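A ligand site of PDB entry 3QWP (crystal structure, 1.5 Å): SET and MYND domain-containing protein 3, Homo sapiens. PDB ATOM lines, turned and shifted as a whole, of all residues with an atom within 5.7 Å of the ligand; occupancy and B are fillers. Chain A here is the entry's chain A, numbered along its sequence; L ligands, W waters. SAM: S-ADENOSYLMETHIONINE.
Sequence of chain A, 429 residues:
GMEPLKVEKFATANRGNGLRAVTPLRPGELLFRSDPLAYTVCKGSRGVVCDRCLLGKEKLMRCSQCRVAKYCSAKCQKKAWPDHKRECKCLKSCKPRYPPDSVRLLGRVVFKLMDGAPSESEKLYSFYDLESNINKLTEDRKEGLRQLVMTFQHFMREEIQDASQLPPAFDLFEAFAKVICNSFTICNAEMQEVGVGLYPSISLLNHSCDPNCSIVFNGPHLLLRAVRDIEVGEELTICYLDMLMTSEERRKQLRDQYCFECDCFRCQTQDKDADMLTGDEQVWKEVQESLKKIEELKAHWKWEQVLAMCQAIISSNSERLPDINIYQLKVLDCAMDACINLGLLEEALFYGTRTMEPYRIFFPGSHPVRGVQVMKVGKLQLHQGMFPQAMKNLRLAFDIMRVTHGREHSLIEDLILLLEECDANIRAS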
ATOM      1  N   ASN A  14     -26.521 -18.021   9.596  1.00  0.00           N
ATOM      2  CA  ASN A  14     -27.297 -19.076   8.959  1.00  0.00           C
ATOM      3  C   ASN A  14     -26.539 -19.990   8.017  1.00  0.00           C
ATOM      4  O   ASN A  14     -27.124 -20.665   7.164  1.00  0.00           O
ATOM      5  CB  ASN A  14     -28.566 -18.517   8.274  1.00  0.00           C
ATOM      6  CG  ASN A  14     -28.260 -17.527   7.178  1.00  0.00           C
ATOM      7  OD1 ASN A  14     -27.259 -17.626   6.454  1.00  0.00           O
ATOM      8  ND2 ASN A  14     -29.146 -16.537   7.028  1.00  0.00           N
ATOM      9  N   ARG A  15     -25.232 -19.886   8.054  1.00  0.00           N
ATOM     10  CA  ARG A  15     -24.446 -20.761   7.194  1.00  0.00           C
ATOM     11  C   ARG A  15     -23.254 -21.397   7.907  1.00  0.00           C
ATOM     12  O   ARG A  15     -22.159 -21.592   7.335  1.00  0.00           O
ATOM     13  CB  ARG A  15     -24.077 -20.107   5.866  1.00  0.00           C
ATOM     14  CG  ARG A  15     -23.523 -18.772   5.937  1.00  0.00           C
ATOM     15  CD  ARG A  15     -23.774 -18.098   4.583  1.00  0.00           C
ATOM     16  NE  ARG A  15     -22.924 -16.921   4.386  1.00  0.00           N
ATOM     17  CZ  ARG A  15     -23.062 -16.063   3.368  1.00  0.00           C
ATOM     18  NH1 ARG A  15     -24.060 -16.206   2.508  1.00  0.00           N
ATOM     19  NH2 ARG A  15     -22.232 -15.027   3.258  1.00  0.00           N
ATOM     20  N   GLY A  16     -23.475 -21.730   9.149  1.00  0.00           N
ATOM     21  CA  GLY A  16     -22.474 -22.447   9.900  1.00  0.00           C
ATOM     22  C   GLY A  16     -21.307 -21.583  10.323  1.00  0.00           C
ATOM     23  O   GLY A  16     -21.433 -20.382  10.531  1.00  0.00           O
ATOM     24  N   ASN A  17     -20.116 -22.163  10.360  1.00  0.00           N
ATOM     25  CA  ASN A  17     -18.941 -21.352  10.615  1.00  0.00           C
ATOM     26  C   ASN A  17     -18.492 -20.666   9.346  1.00  0.00           C
ATOM     27  O   ASN A  17     -18.850 -21.106   8.229  1.00  0.00           O
ATOM     28  CB  ASN A  17     -17.777 -22.203  11.187  1.00  0.00           C
ATOM     29  CG  ASN A  17     -18.154 -22.836  12.510  1.00  0.00           C
ATOM     30  OD1 ASN A  17     -18.006 -24.062  12.704  1.00  0.00           O
ATOM     31  ND2 ASN A  17     -18.733 -22.031  13.410  1.00  0.00           N
ATOM     32  N   GLY A  18     -17.768 -19.576   9.505  1.00  0.00           N
ATOM     33  CA  GLY A  18     -17.197 -18.882   8.342  1.00  0.00           C
ATOM     34  C   GLY A  18     -15.929 -18.165   8.736  1.00  0.00           C
ATOM     35  O   GLY A  18     -15.413 -18.358   9.862  1.00  0.00           O
ATOM     36  N   TYR A 125      -9.017 -24.533  11.561  1.00  0.00           N
ATOM     37  CA  TYR A 125     -10.114 -25.470  11.500  1.00  0.00           C
ATOM     38  C   TYR A 125      -9.547 -26.813  11.109  1.00  0.00           C
ATOM     39  O   TYR A 125      -8.670 -26.880  10.233  1.00  0.00           O
ATOM     40  CB  TYR A 125     -11.062 -25.007  10.391  1.00  0.00           C
ATOM     41  CG  TYR A 125     -12.555 -25.367  10.517  1.00  0.00           C
ATOM     42  CD1 TYR A 125     -13.287 -25.073  11.683  1.00  0.00           C
ATOM     43  CD2 TYR A 125     -13.273 -25.797   9.384  1.00  0.00           C
ATOM     44  CE1 TYR A 125     -14.654 -25.238  11.762  1.00  0.00           C
ATOM     45  CE2 TYR A 125     -14.657 -25.947   9.429  1.00  0.00           C
ATOM     46  CZ  TYR A 125     -15.346 -25.700  10.640  1.00  0.00           C
ATOM     47  OH  TYR A 125     -16.725 -25.749  10.631  1.00  0.00           O
ATOM     48  N   ASP A 129     -13.445 -30.832  12.565  1.00  0.00           N
ATOM     49  CA  ASP A 129     -14.393 -29.744  12.602  1.00  0.00           C
ATOM     50  C   ASP A 129     -15.228 -29.648  11.321  1.00  0.00           C
ATOM     51  O   ASP A 129     -16.251 -28.963  11.321  1.00  0.00           O
ATOM     52  CB  ASP A 129     -13.670 -28.413  12.777  1.00  0.00           C
ATOM     53  CG  ASP A 129     -12.899 -28.302  14.056  1.00  0.00           C
ATOM     54  OD1 ASP A 129     -13.379 -28.774  15.133  1.00  0.00           O
ATOM     55  OD2 ASP A 129     -11.836 -27.598  13.989  1.00  0.00           O
ATOM     56  N   LEU A 130     -14.788 -30.275  10.233  1.00  0.00           N
ATOM     57  CA  LEU A 130     -15.432 -29.999   8.946  1.00  0.00           C
ATOM     58  C   LEU A 130     -16.920 -30.357   8.959  1.00  0.00           C
ATOM     59  O   LEU A 130     -17.373 -31.350   9.573  1.00  0.00           O
ATOM     60  CB  LEU A 130     -14.758 -30.780   7.812  1.00  0.00           C
ATOM     61  CG  LEU A 130     -13.317 -30.431   7.515  1.00  0.00           C
ATOM     62  CD1 LEU A 130     -12.730 -31.403   6.436  1.00  0.00           C
ATOM     63  CD2 LEU A 130     -13.255 -28.956   7.037  1.00  0.00           C
ATOM     64  N   GLU A 131     -17.653 -29.576   8.176  1.00  0.00           N
ATOM     65  CA  GLU A 131     -19.093 -29.809   7.979  1.00  0.00           C
ATOM     66  C   GLU A 131     -19.335 -31.114   7.183  1.00  0.00           C
ATOM     67  O   GLU A 131     -18.674 -31.351   6.151  1.00  0.00           O
ATOM     68  CB  GLU A 131     -19.664 -28.630   7.210  1.00  0.00           C
ATOM     69  CG  GLU A 131     -21.151 -28.754   6.847  1.00  0.00           C
ATOM     70  CD  GLU A 131     -22.022 -28.758   8.080  1.00  0.00           C
ATOM     71  OE1 GLU A 131     -22.155 -27.674   8.731  1.00  0.00           O
ATOM     72  OE2 GLU A 131     -22.553 -29.826   8.453  1.00  0.00           O
ATOM     73  N   ASN A 133     -22.833 -32.171   6.735  1.00  0.00           N
ATOM     74  CA  ASN A 133     -24.224 -32.075   6.228  1.00  0.00           C
ATOM     75  C   ASN A 133     -25.010 -33.375   6.370  1.00  0.00           C
ATOM     76  O   ASN A 133     -25.919 -33.646   5.574  1.00  0.00           O
ATOM     77  CB  ASN A 133     -24.261 -31.616   4.752  1.00  0.00           C
ATOM     78  CG  ASN A 133     -23.912 -30.165   4.609  1.00  0.00           C
ATOM     79  OD1 ASN A 133     -24.447 -29.333   5.341  1.00  0.00           O
ATOM     80  ND2 ASN A 133     -22.918 -29.861   3.795  1.00  0.00           N
ATOM     81  N   LYS A 136     -28.712 -33.496   6.105  1.00  0.00           N
ATOM     82  CA  LYS A 136     -29.342 -33.045   4.842  1.00  0.00           C
ATOM     83  C   LYS A 136     -29.178 -34.023   3.653  1.00  0.00           C
ATOM     84  O   LYS A 136     -29.752 -33.816   2.564  1.00  0.00           O
ATOM     85  CB  LYS A 136     -28.771 -31.671   4.433  1.00  0.00           C
ATOM     86  CG  LYS A 136     -29.239 -30.576   5.374  1.00  0.00           C
ATOM     87  CD  LYS A 136     -28.691 -29.214   4.907  1.00  0.00           C
ATOM     88  CE  LYS A 136     -28.965 -28.154   5.935  1.00  0.00           C
ATOM     89  NZ  LYS A 136     -28.319 -26.888   5.415  1.00  0.00           N
ATOM     90  N   CYS A 181     -18.197 -32.456   0.606  1.00  0.00           N
ATOM     91  CA  CYS A 181     -18.448 -31.013   0.611  1.00  0.00           C
ATOM     92  C   CYS A 181     -17.252 -30.147   0.999  1.00  0.00           C
ATOM     93  O   CYS A 181     -17.413 -28.954   1.142  1.00  0.00           O
ATOM     94  CB  CYS A 181     -19.669 -30.599   1.440  1.00  0.00           C
ATOM     95  SG  CYS A 181     -19.545 -31.042   3.179  1.00  0.00           S
ATOM     96  N   ASN A 182     -16.082 -30.748   1.197  1.00  0.00           N
ATOM     97  CA  ASN A 182     -14.888 -29.966   1.505  1.00  0.00           C
ATOM     98  C   ASN A 182     -13.662 -30.257   0.653  1.00  0.00           C
ATOM     99  O   ASN A 182     -12.591 -29.749   0.923  1.00  0.00           O
ATOM    100  CB  ASN A 182     -14.523 -30.200   2.970  1.00  0.00           C
ATOM    101  CG  ASN A 182     -15.595 -29.665   3.908  1.00  0.00           C
ATOM    102  OD1 ASN A 182     -15.687 -28.450   4.110  1.00  0.00           O
ATOM    103  ND2 ASN A 182     -16.390 -30.544   4.495  1.00  0.00           N
ATOM    104  N   ILE A 202      -9.017 -23.496   4.976  1.00  0.00           N
ATOM    105  CA  ILE A 202      -9.592 -22.794   3.828  1.00  0.00           C
ATOM    106  C   ILE A 202     -11.048 -23.238   3.682  1.00  0.00           C
ATOM    107  O   ILE A 202     -11.864 -22.495   3.117  1.00  0.00           O
ATOM    108  CB  ILE A 202      -8.808 -23.096   2.518  1.00  0.00           C
ATOM    109  CG1 ILE A 202      -7.322 -22.859   2.771  1.00  0.00           C
ATOM    110  CG2 ILE A 202      -9.390 -22.279   1.317  1.00  0.00           C
ATOM    111  CD1 ILE A 202      -6.993 -21.417   3.188  1.00  0.00           C
ATOM    112  N   SER A 203     -11.386 -24.415   4.235  1.00  0.00           N
ATOM    113  CA  SER A 203     -12.766 -24.861   4.210  1.00  0.00           C
ATOM    114  C   SER A 203     -13.710 -24.037   5.067  1.00  0.00           C
ATOM    115  O   SER A 203     -14.928 -24.188   4.932  1.00  0.00           O
ATOM    116  CB  SER A 203     -12.939 -26.324   4.577  1.00  0.00           C
ATOM    117  OG  SER A 203     -12.437 -27.124   3.543  1.00  0.00           O
ATOM    118  N   LEU A 204     -13.199 -23.080   5.848  1.00  0.00           N
ATOM    119  CA  LEU A 204     -14.065 -22.136   6.545  1.00  0.00           C
ATOM    120  C   LEU A 204     -14.767 -21.201   5.620  1.00  0.00           C
ATOM    121  O   LEU A 204     -15.825 -20.673   5.995  1.00  0.00           O
ATOM    122  CB  LEU A 204     -13.296 -21.308   7.573  1.00  0.00           C
ATOM    123  CG  LEU A 204     -13.133 -22.084   8.868  1.00  0.00           C
ATOM    124  CD1 LEU A 204     -12.093 -21.274   9.700  1.00  0.00           C
ATOM    125  CD2 LEU A 204     -14.458 -22.284   9.611  1.00  0.00           C
ATOM    126  N   LEU A 205     -14.260 -21.015   4.409  1.00  0.00           N
ATOM    127  CA  LEU A 205     -14.869 -19.986   3.556  1.00  0.00           C
ATOM    128  C   LEU A 205     -16.186 -20.480   2.992  1.00  0.00           C
ATOM    129  O   LEU A 205     -16.224 -21.503   2.291  1.00  0.00           O
ATOM    130  CB  LEU A 205     -13.942 -19.648   2.383  1.00  0.00           C
ATOM    131  CG  LEU A 205     -12.638 -18.966   2.780  1.00  0.00           C
ATOM    132  CD1 LEU A 205     -11.540 -19.360   1.806  1.00  0.00           C
ATOM    133  CD2 LEU A 205     -12.847 -17.467   2.698  1.00  0.00           C
ATOM    134  N   ASN A 206     -17.253 -19.711   3.199  1.00  0.00           N
ATOM    135  CA  ASN A 206     -18.508 -19.990   2.534  1.00  0.00           C
ATOM    136  C   ASN A 206     -18.560 -19.458   1.115  1.00  0.00           C
ATOM    137  O   ASN A 206     -17.630 -18.784   0.678  1.00  0.00           O
ATOM    138  CB  ASN A 206     -19.620 -19.353   3.411  1.00  0.00           C
ATOM    139  CG  ASN A 206     -19.849 -20.156   4.666  1.00  0.00           C
ATOM    140  OD1 ASN A 206     -19.986 -21.389   4.593  1.00  0.00           O
ATOM    141  ND2 ASN A 206     -19.966 -19.495   5.803  1.00  0.00           N
ATOM    142  N   HIS A 207     -19.524 -19.971   0.361  1.00  0.00           N
ATOM    143  CA  HIS A 207     -19.683 -19.682  -1.045  1.00  0.00           C
ATOM    144  C   HIS A 207     -20.402 -18.387  -1.353  1.00  0.00           C
ATOM    145  O   HIS A 207     -21.395 -18.053  -0.713  1.00  0.00           O
ATOM    146  CB  HIS A 207     -20.493 -20.844  -1.657  1.00  0.00           C
ATOM    147  CG  HIS A 207     -20.971 -20.553  -3.051  1.00  0.00           C
ATOM    148  ND1 HIS A 207     -20.177 -20.713  -4.170  1.00  0.00           N
ATOM    149  CD2 HIS A 207     -22.123 -19.978  -3.480  1.00  0.00           C
ATOM    150  CE1 HIS A 207     -20.837 -20.319  -5.247  1.00  0.00           C
ATOM    151  NE2 HIS A 207     -22.050 -19.904  -4.859  1.00  0.00           N
ATOM    152  N   SER A 208     -19.968 -17.733  -2.433  1.00  0.00           N
ATOM    153  CA  SER A 208     -20.816 -16.748  -3.096  1.00  0.00           C
ATOM    154  C   SER A 208     -20.625 -16.825  -4.583  1.00  0.00           C
ATOM    155  O   SER A 208     -19.503 -17.070  -5.082  1.00  0.00           O
ATOM    156  CB  SER A 208     -20.355 -15.373  -2.637  1.00  0.00           C
ATOM    157  OG  SER A 208     -21.020 -14.362  -3.385  1.00  0.00           O
ATOM    158  N   TYR A 240     -17.428 -21.455  -5.155  1.00  0.00           N
ATOM    159  CA  TYR A 240     -17.090 -22.899  -5.226  1.00  0.00           C
ATOM    160  C   TYR A 240     -17.132 -23.428  -6.632  1.00  0.00           C
ATOM    161  O   TYR A 240     -16.687 -24.560  -6.902  1.00  0.00           O
ATOM    162  CB  TYR A 240     -18.084 -23.707  -4.374  1.00  0.00           C
ATOM    163  CG  TYR A 240     -18.086 -23.494  -2.869  1.00  0.00           C
ATOM    164  CD1 TYR A 240     -17.185 -22.608  -2.228  1.00  0.00           C
ATOM    165  CD2 TYR A 240     -19.012 -24.202  -2.080  1.00  0.00           C
ATOM    166  CE1 TYR A 240     -17.166 -22.482  -0.831  1.00  0.00           C
ATOM    167  CE2 TYR A 240     -19.033 -24.081  -0.704  1.00  0.00           C
ATOM    168  CZ  TYR A 240     -18.107 -23.213  -0.072  1.00  0.00           C
ATOM    169  OH  TYR A 240     -18.140 -23.087   1.297  1.00  0.00           O
ATOM    170  N   GLN A 257     -23.955 -31.332  -4.068  1.00  0.00           N
ATOM    171  CA  GLN A 257     -22.634 -31.517  -3.491  1.00  0.00           C
ATOM    172  C   GLN A 257     -22.598 -30.875  -2.109  1.00  0.00           C
ATOM    173  O   GLN A 257     -21.893 -31.359  -1.184  1.00  0.00           O
ATOM    174  CB  GLN A 257     -21.548 -30.899  -4.398  1.00  0.00           C
ATOM    175  CG  GLN A 257     -20.164 -31.051  -3.790  1.00  0.00           C
ATOM    176  CD  GLN A 257     -19.053 -30.667  -4.733  1.00  0.00           C
ATOM    177  OE1 GLN A 257     -19.272 -30.331  -5.927  1.00  0.00           O
ATOM    178  NE2 GLN A 257     -17.826 -30.740  -4.222  1.00  0.00           N
ATOM    179  N   TYR A 258     -23.204 -29.690  -1.975  1.00  0.00           N
ATOM    180  CA  TYR A 258     -22.999 -28.885  -0.736  1.00  0.00           C
ATOM    181  C   TYR A 258     -24.238 -28.750   0.152  1.00  0.00           C
ATOM    182  O   TYR A 258     -24.203 -28.054   1.141  1.00  0.00           O
ATOM    183  CB  TYR A 258     -22.476 -27.479  -1.085  1.00  0.00           C
ATOM    184  CG  TYR A 258     -21.158 -27.544  -1.796  1.00  0.00           C
ATOM    185  CD1 TYR A 258     -19.982 -27.694  -1.072  1.00  0.00           C
ATOM    186  CD2 TYR A 258     -21.079 -27.375  -3.173  1.00  0.00           C
ATOM    187  CE1 TYR A 258     -18.770 -27.733  -1.744  1.00  0.00           C
ATOM    188  CE2 TYR A 258     -19.839 -27.391  -3.850  1.00  0.00           C
ATOM    189  CZ  TYR A 258     -18.720 -27.550  -3.105  1.00  0.00           C
ATOM    190  OH  TYR A 258     -17.487 -27.558  -3.782  1.00  0.00           O
ATOM    191  N   CYS A 259     -25.348 -29.310  -0.279  1.00  0.00           N
ATOM    192  CA  CYS A 259     -26.625 -29.243   0.482  1.00  0.00           C
ATOM    193  C   CYS A 259     -26.992 -27.839   0.961  1.00  0.00           C
ATOM    194  O   CYS A 259     -27.366 -27.645   2.135  1.00  0.00           O
ATOM    195  CB  CYS A 259     -26.559 -30.144   1.738  1.00  0.00           C
ATOM    196  SG  CYS A 259     -26.345 -31.873   1.351  1.00  0.00           S
ATOM    197  N   PHE A 260     -26.941 -26.841   0.054  1.00  0.00           N
ATOM    198  CA  PHE A 260     -27.637 -25.576   0.325  1.00  0.00           C
ATOM    199  C   PHE A 260     -28.249 -24.934  -0.914  1.00  0.00           C
ATOM    200  O   PHE A 260     -27.977 -25.370  -2.038  1.00  0.00           O
ATOM    201  CB  PHE A 260     -26.752 -24.588   1.090  1.00  0.00           C
ATOM    202  CG  PHE A 260     -25.656 -23.943   0.243  1.00  0.00           C
ATOM    203  CD1 PHE A 260     -25.871 -22.693  -0.332  1.00  0.00           C
ATOM    204  CD2 PHE A 260     -24.434 -24.600   0.023  1.00  0.00           C
ATOM    205  CE1 PHE A 260     -24.836 -22.090  -1.111  1.00  0.00           C
ATOM    206  CE2 PHE A 260     -23.421 -24.005  -0.735  1.00  0.00           C
ATOM    207  CZ  PHE A 260     -23.613 -22.751  -1.289  1.00  0.00           C
ATOM    208  N   GLU A 261     -29.141 -23.981  -0.635  1.00  0.00           N
ATOM    209  CA  GLU A 261     -29.831 -23.170  -1.629  1.00  0.00           C
ATOM    210  C   GLU A 261     -29.229 -21.771  -1.546  1.00  0.00           C
ATOM    211  O   GLU A 261     -29.128 -21.199  -0.463  1.00  0.00           O
ATOM    212  CB  GLU A 261     -31.336 -23.103  -1.249  1.00  0.00           C
ATOM    213  CG  GLU A 261     -31.954 -24.447  -0.630  1.00  0.00           C
ATOM    214  CD  GLU A 261     -32.043 -25.529  -1.656  1.00  0.00           C
ATOM    215  OE1 GLU A 261     -31.892 -25.178  -2.867  1.00  0.00           O
ATOM    216  OE2 GLU A 261     -32.330 -26.720  -1.311  1.00  0.00           O
ATOM    217  N   CYS A 262     -28.574 -21.326  -2.620  1.00  0.00           N
ATOM    218  CA  CYS A 262     -27.813 -20.081  -2.553  1.00  0.00           C
ATOM    219  C   CYS A 262     -28.761 -18.928  -2.766  1.00  0.00           C
ATOM    220  O   CYS A 262     -29.519 -18.920  -3.736  1.00  0.00           O
ATOM    221  CB  CYS A 262     -26.711 -20.062  -3.644  1.00  0.00           C
ATOM    222  SG  CYS A 262     -25.750 -18.495  -3.770  1.00  0.00           S
HETATM  223  N   SAM L   1     -20.089 -23.253   6.747  1.00  0.00           N
HETATM  224  CA  SAM L   1     -18.950 -24.251   6.695  1.00  0.00           C
HETATM  225  C   SAM L   1     -18.669 -24.850   8.055  1.00  0.00           C
HETATM  226  O   SAM L   1     -19.422 -24.522   8.990  1.00  0.00           O
HETATM  227  OXT SAM L   1     -17.769 -25.678   8.235  1.00  0.00           O
HETATM  228  CB  SAM L   1     -17.694 -23.750   5.988  1.00  0.00           C
HETATM  229  CG  SAM L   1     -17.836 -23.868   4.437  1.00  0.00           C
HETATM  230  SD  SAM L   1     -17.840 -25.646   3.956  1.00  0.00           S
HETATM  231  CE  SAM L   1     -16.508 -25.632   2.719  1.00  0.00           C
HETATM  232  C5' SAM L   1     -19.254 -25.733   2.814  1.00  0.00           C
HETATM  233  C4' SAM L   1     -20.572 -25.851   3.565  1.00  0.00           C
HETATM  234  O4' SAM L   1     -20.896 -24.588   4.122  1.00  0.00           O
HETATM  235  C3' SAM L   1     -21.742 -26.136   2.621  1.00  0.00           C
HETATM  236  O3' SAM L   1     -21.923 -27.531   2.406  1.00  0.00           O
HETATM  237  C2' SAM L   1     -22.906 -25.529   3.390  1.00  0.00           C
HETATM  238  O2' SAM L   1     -23.223 -26.293   4.571  1.00  0.00           O
HETATM  239  C1' SAM L   1     -22.276 -24.248   3.944  1.00  0.00           C
HETATM  240  N9  SAM L   1     -22.337 -23.114   2.959  1.00  0.00           N
HETATM  241  C8  SAM L   1     -21.304 -22.569   2.224  1.00  0.00           C
HETATM  242  N7  SAM L   1     -21.735 -21.485   1.586  1.00  0.00           N
HETATM  243  C5  SAM L   1     -23.031 -21.248   1.937  1.00  0.00           C
HETATM  244  C6  SAM L   1     -23.961 -20.317   1.526  1.00  0.00           C
HETATM  245  N6  SAM L   1     -23.690 -19.294   0.696  1.00  0.00           N
HETATM  246  N1  SAM L   1     -25.229 -20.433   2.020  1.00  0.00           N
HETATM  247  C2  SAM L   1     -25.570 -21.426   2.875  1.00  0.00           C
HETATM  248  N3  SAM L   1     -24.674 -22.382   3.270  1.00  0.00           N
HETATM  249  C4  SAM L   1     -23.423 -22.268   2.790  1.00  0.00           C
HETATM  250  O   HOH W   1     -16.371 -27.533   6.699  1.00  0.00           O
HETATM  251  O   HOH W   2     -25.942 -27.015   4.308  1.00  0.00           O
HETATM  252  O   HOH W   3     -22.208 -25.127   7.326  1.00  0.00           O
HETATM  253  O   HOH W   4     -27.726 -19.193   0.912  1.00  0.00           O
HETATM  254  O   HOH W   5     -25.649 -17.399  -0.705  1.00  0.00           O
HETATM  255  O   HOH W   6     -26.231 -24.050   4.956  1.00  0.00           O
HETATM  256  O   HOH W   7     -20.293 -26.337  10.810  1.00  0.00           O
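OXT of the ligand lies within hydrogen-bond range of OH of Tyr 125.
An oxygen (O3') of the ligand sits at hydrogen-bond distance from the backbone carbonyl oxygen of Tyr 258 (2.7 Å).
O of Arg 15 sits at hydrogen-bond distance from N of the ligand, 2.7 Å away.
The backbone NH (N) of Asn 17 lies within hydrogen-bond range of an oxygen (O) of the ligand (2.8 Å).
A nitrogen (N) of the ligand sits at hydrogen-bond distance from the backbone carbonyl oxygen of Asn 17 (2.9 Å).
The side-chain amide oxygen (OD1) of Asn 206 lies within hydrogen-bond range of a nitrogen (N) of the ligand (2.9 Å).
O3' of the ligand is in hydrogen-bond range of ND2 of Asn 133, at 2.9 Å.
N of His 207 lies within hydrogen-bond range of N7 of the ligand (2.9 Å).
O of His 207 lies within hydrogen-bond range of N6 of the ligand (3.0 Å).
The side-chain amide nitrogen (ND2) of Asn 133 lies within hydrogen-bond range of the backbone carbonyl oxygen (O) of Tyr 258 (3.5 Å).
The backbone carbonyl oxygen (O) of Arg 15 lies within hydrogen-bond range of the side-chain amide nitrogen (ND2) of Asn 206, at 3.4 Å.
ND2 of Asn 206 lies within hydrogen-bond range of O of Asn 17 (3.1 Å).
N of Asn 133 sits at hydrogen-bond distance from OE2 of Glu 131 (2.9 Å).
The side-chain amide nitrogen of Asn 133 sits at hydrogen-bond distance from the side-chain sulfur of Cys 181, 3.6 Å away.
A ring nitrogen (ND1) of His 207 sits at hydrogen-bond distance from the backbone NH of Tyr 240.
The backbone carbonyl oxygen (O) of Glu 131 lies within hydrogen-bond range of the side-chain amide nitrogen (ND2) of Asn 182, 2.9 Å away.
The side-chain amide nitrogen (ND2) of Asn 182 sits at hydrogen-bond distance from the side-chain sulfur (SG) of Cys 181 (3.5 Å).
The side-chain amide oxygen (OD1) of Asn 182 sits close to a sulfur (SD) of the ligand (3.5 Å).
The backbone carbonyl oxygen (O) of Ser 203 sits close to a sulfur (SD) of the ligand (3.4 Å).
OH of Tyr 240 sits close to SD of the ligand (3.7 Å).
Gly 16 touches the ligand (C to O, 3.7 Å).
CB of Glu 131 touches OXT of the ligand, at 3.7 Å.
O of Cys 181 touches CE of the ligand (3.8 Å).
O of Leu 204 touches CB of the ligand (3.6 Å).
Leu 205 touches the ligand (O to CG, 3.6 Å).
Phe 260 touches the ligand (CE1 to C6, 3.3 Å).
Hydrophobic or aromatic side chains within 4 Å of the ligand: Tyr 125, His 207, Tyr 240, Tyr 258 and Phe 260.
Of the 27 residues printed, 16 come within 4 Å of the ligand.
The nearest printed residue that does not touch the ligand is Asn 14 (4.6 Å).
Water W7 lies within hydrogen-bond range of an oxygen (O) of the ligand (2.7 Å) and the side-chain carboxylate (OE1) of Glu 131 (3.1 Å).
Water W1 lies within hydrogen-bond range of OXT of the ligand, N of Glu 131 and OD1 of Asn 182.
Water W2 lies within hydrogen-bond range of the side-chain amino group (NZ) of Lys 136 (2.6 Å), the backbone carbonyl oxygen (O) of Cys 259 (2.7 Å), an oxygen (O2') of the ligand (2.8 Å) and the side-chain amide oxygen (OD1) of Asn 133 (2.9 Å).
Water W3 lies within hydrogen-bond range of N of the ligand (2.9 Å) and OE1 of Glu 131 (2.9 Å).
Water W4 lies within hydrogen-bond range of the backbone carbonyl oxygen of Glu 261 (2.8 Å) and a nitrogen (N1) of the ligand (3.0 Å).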
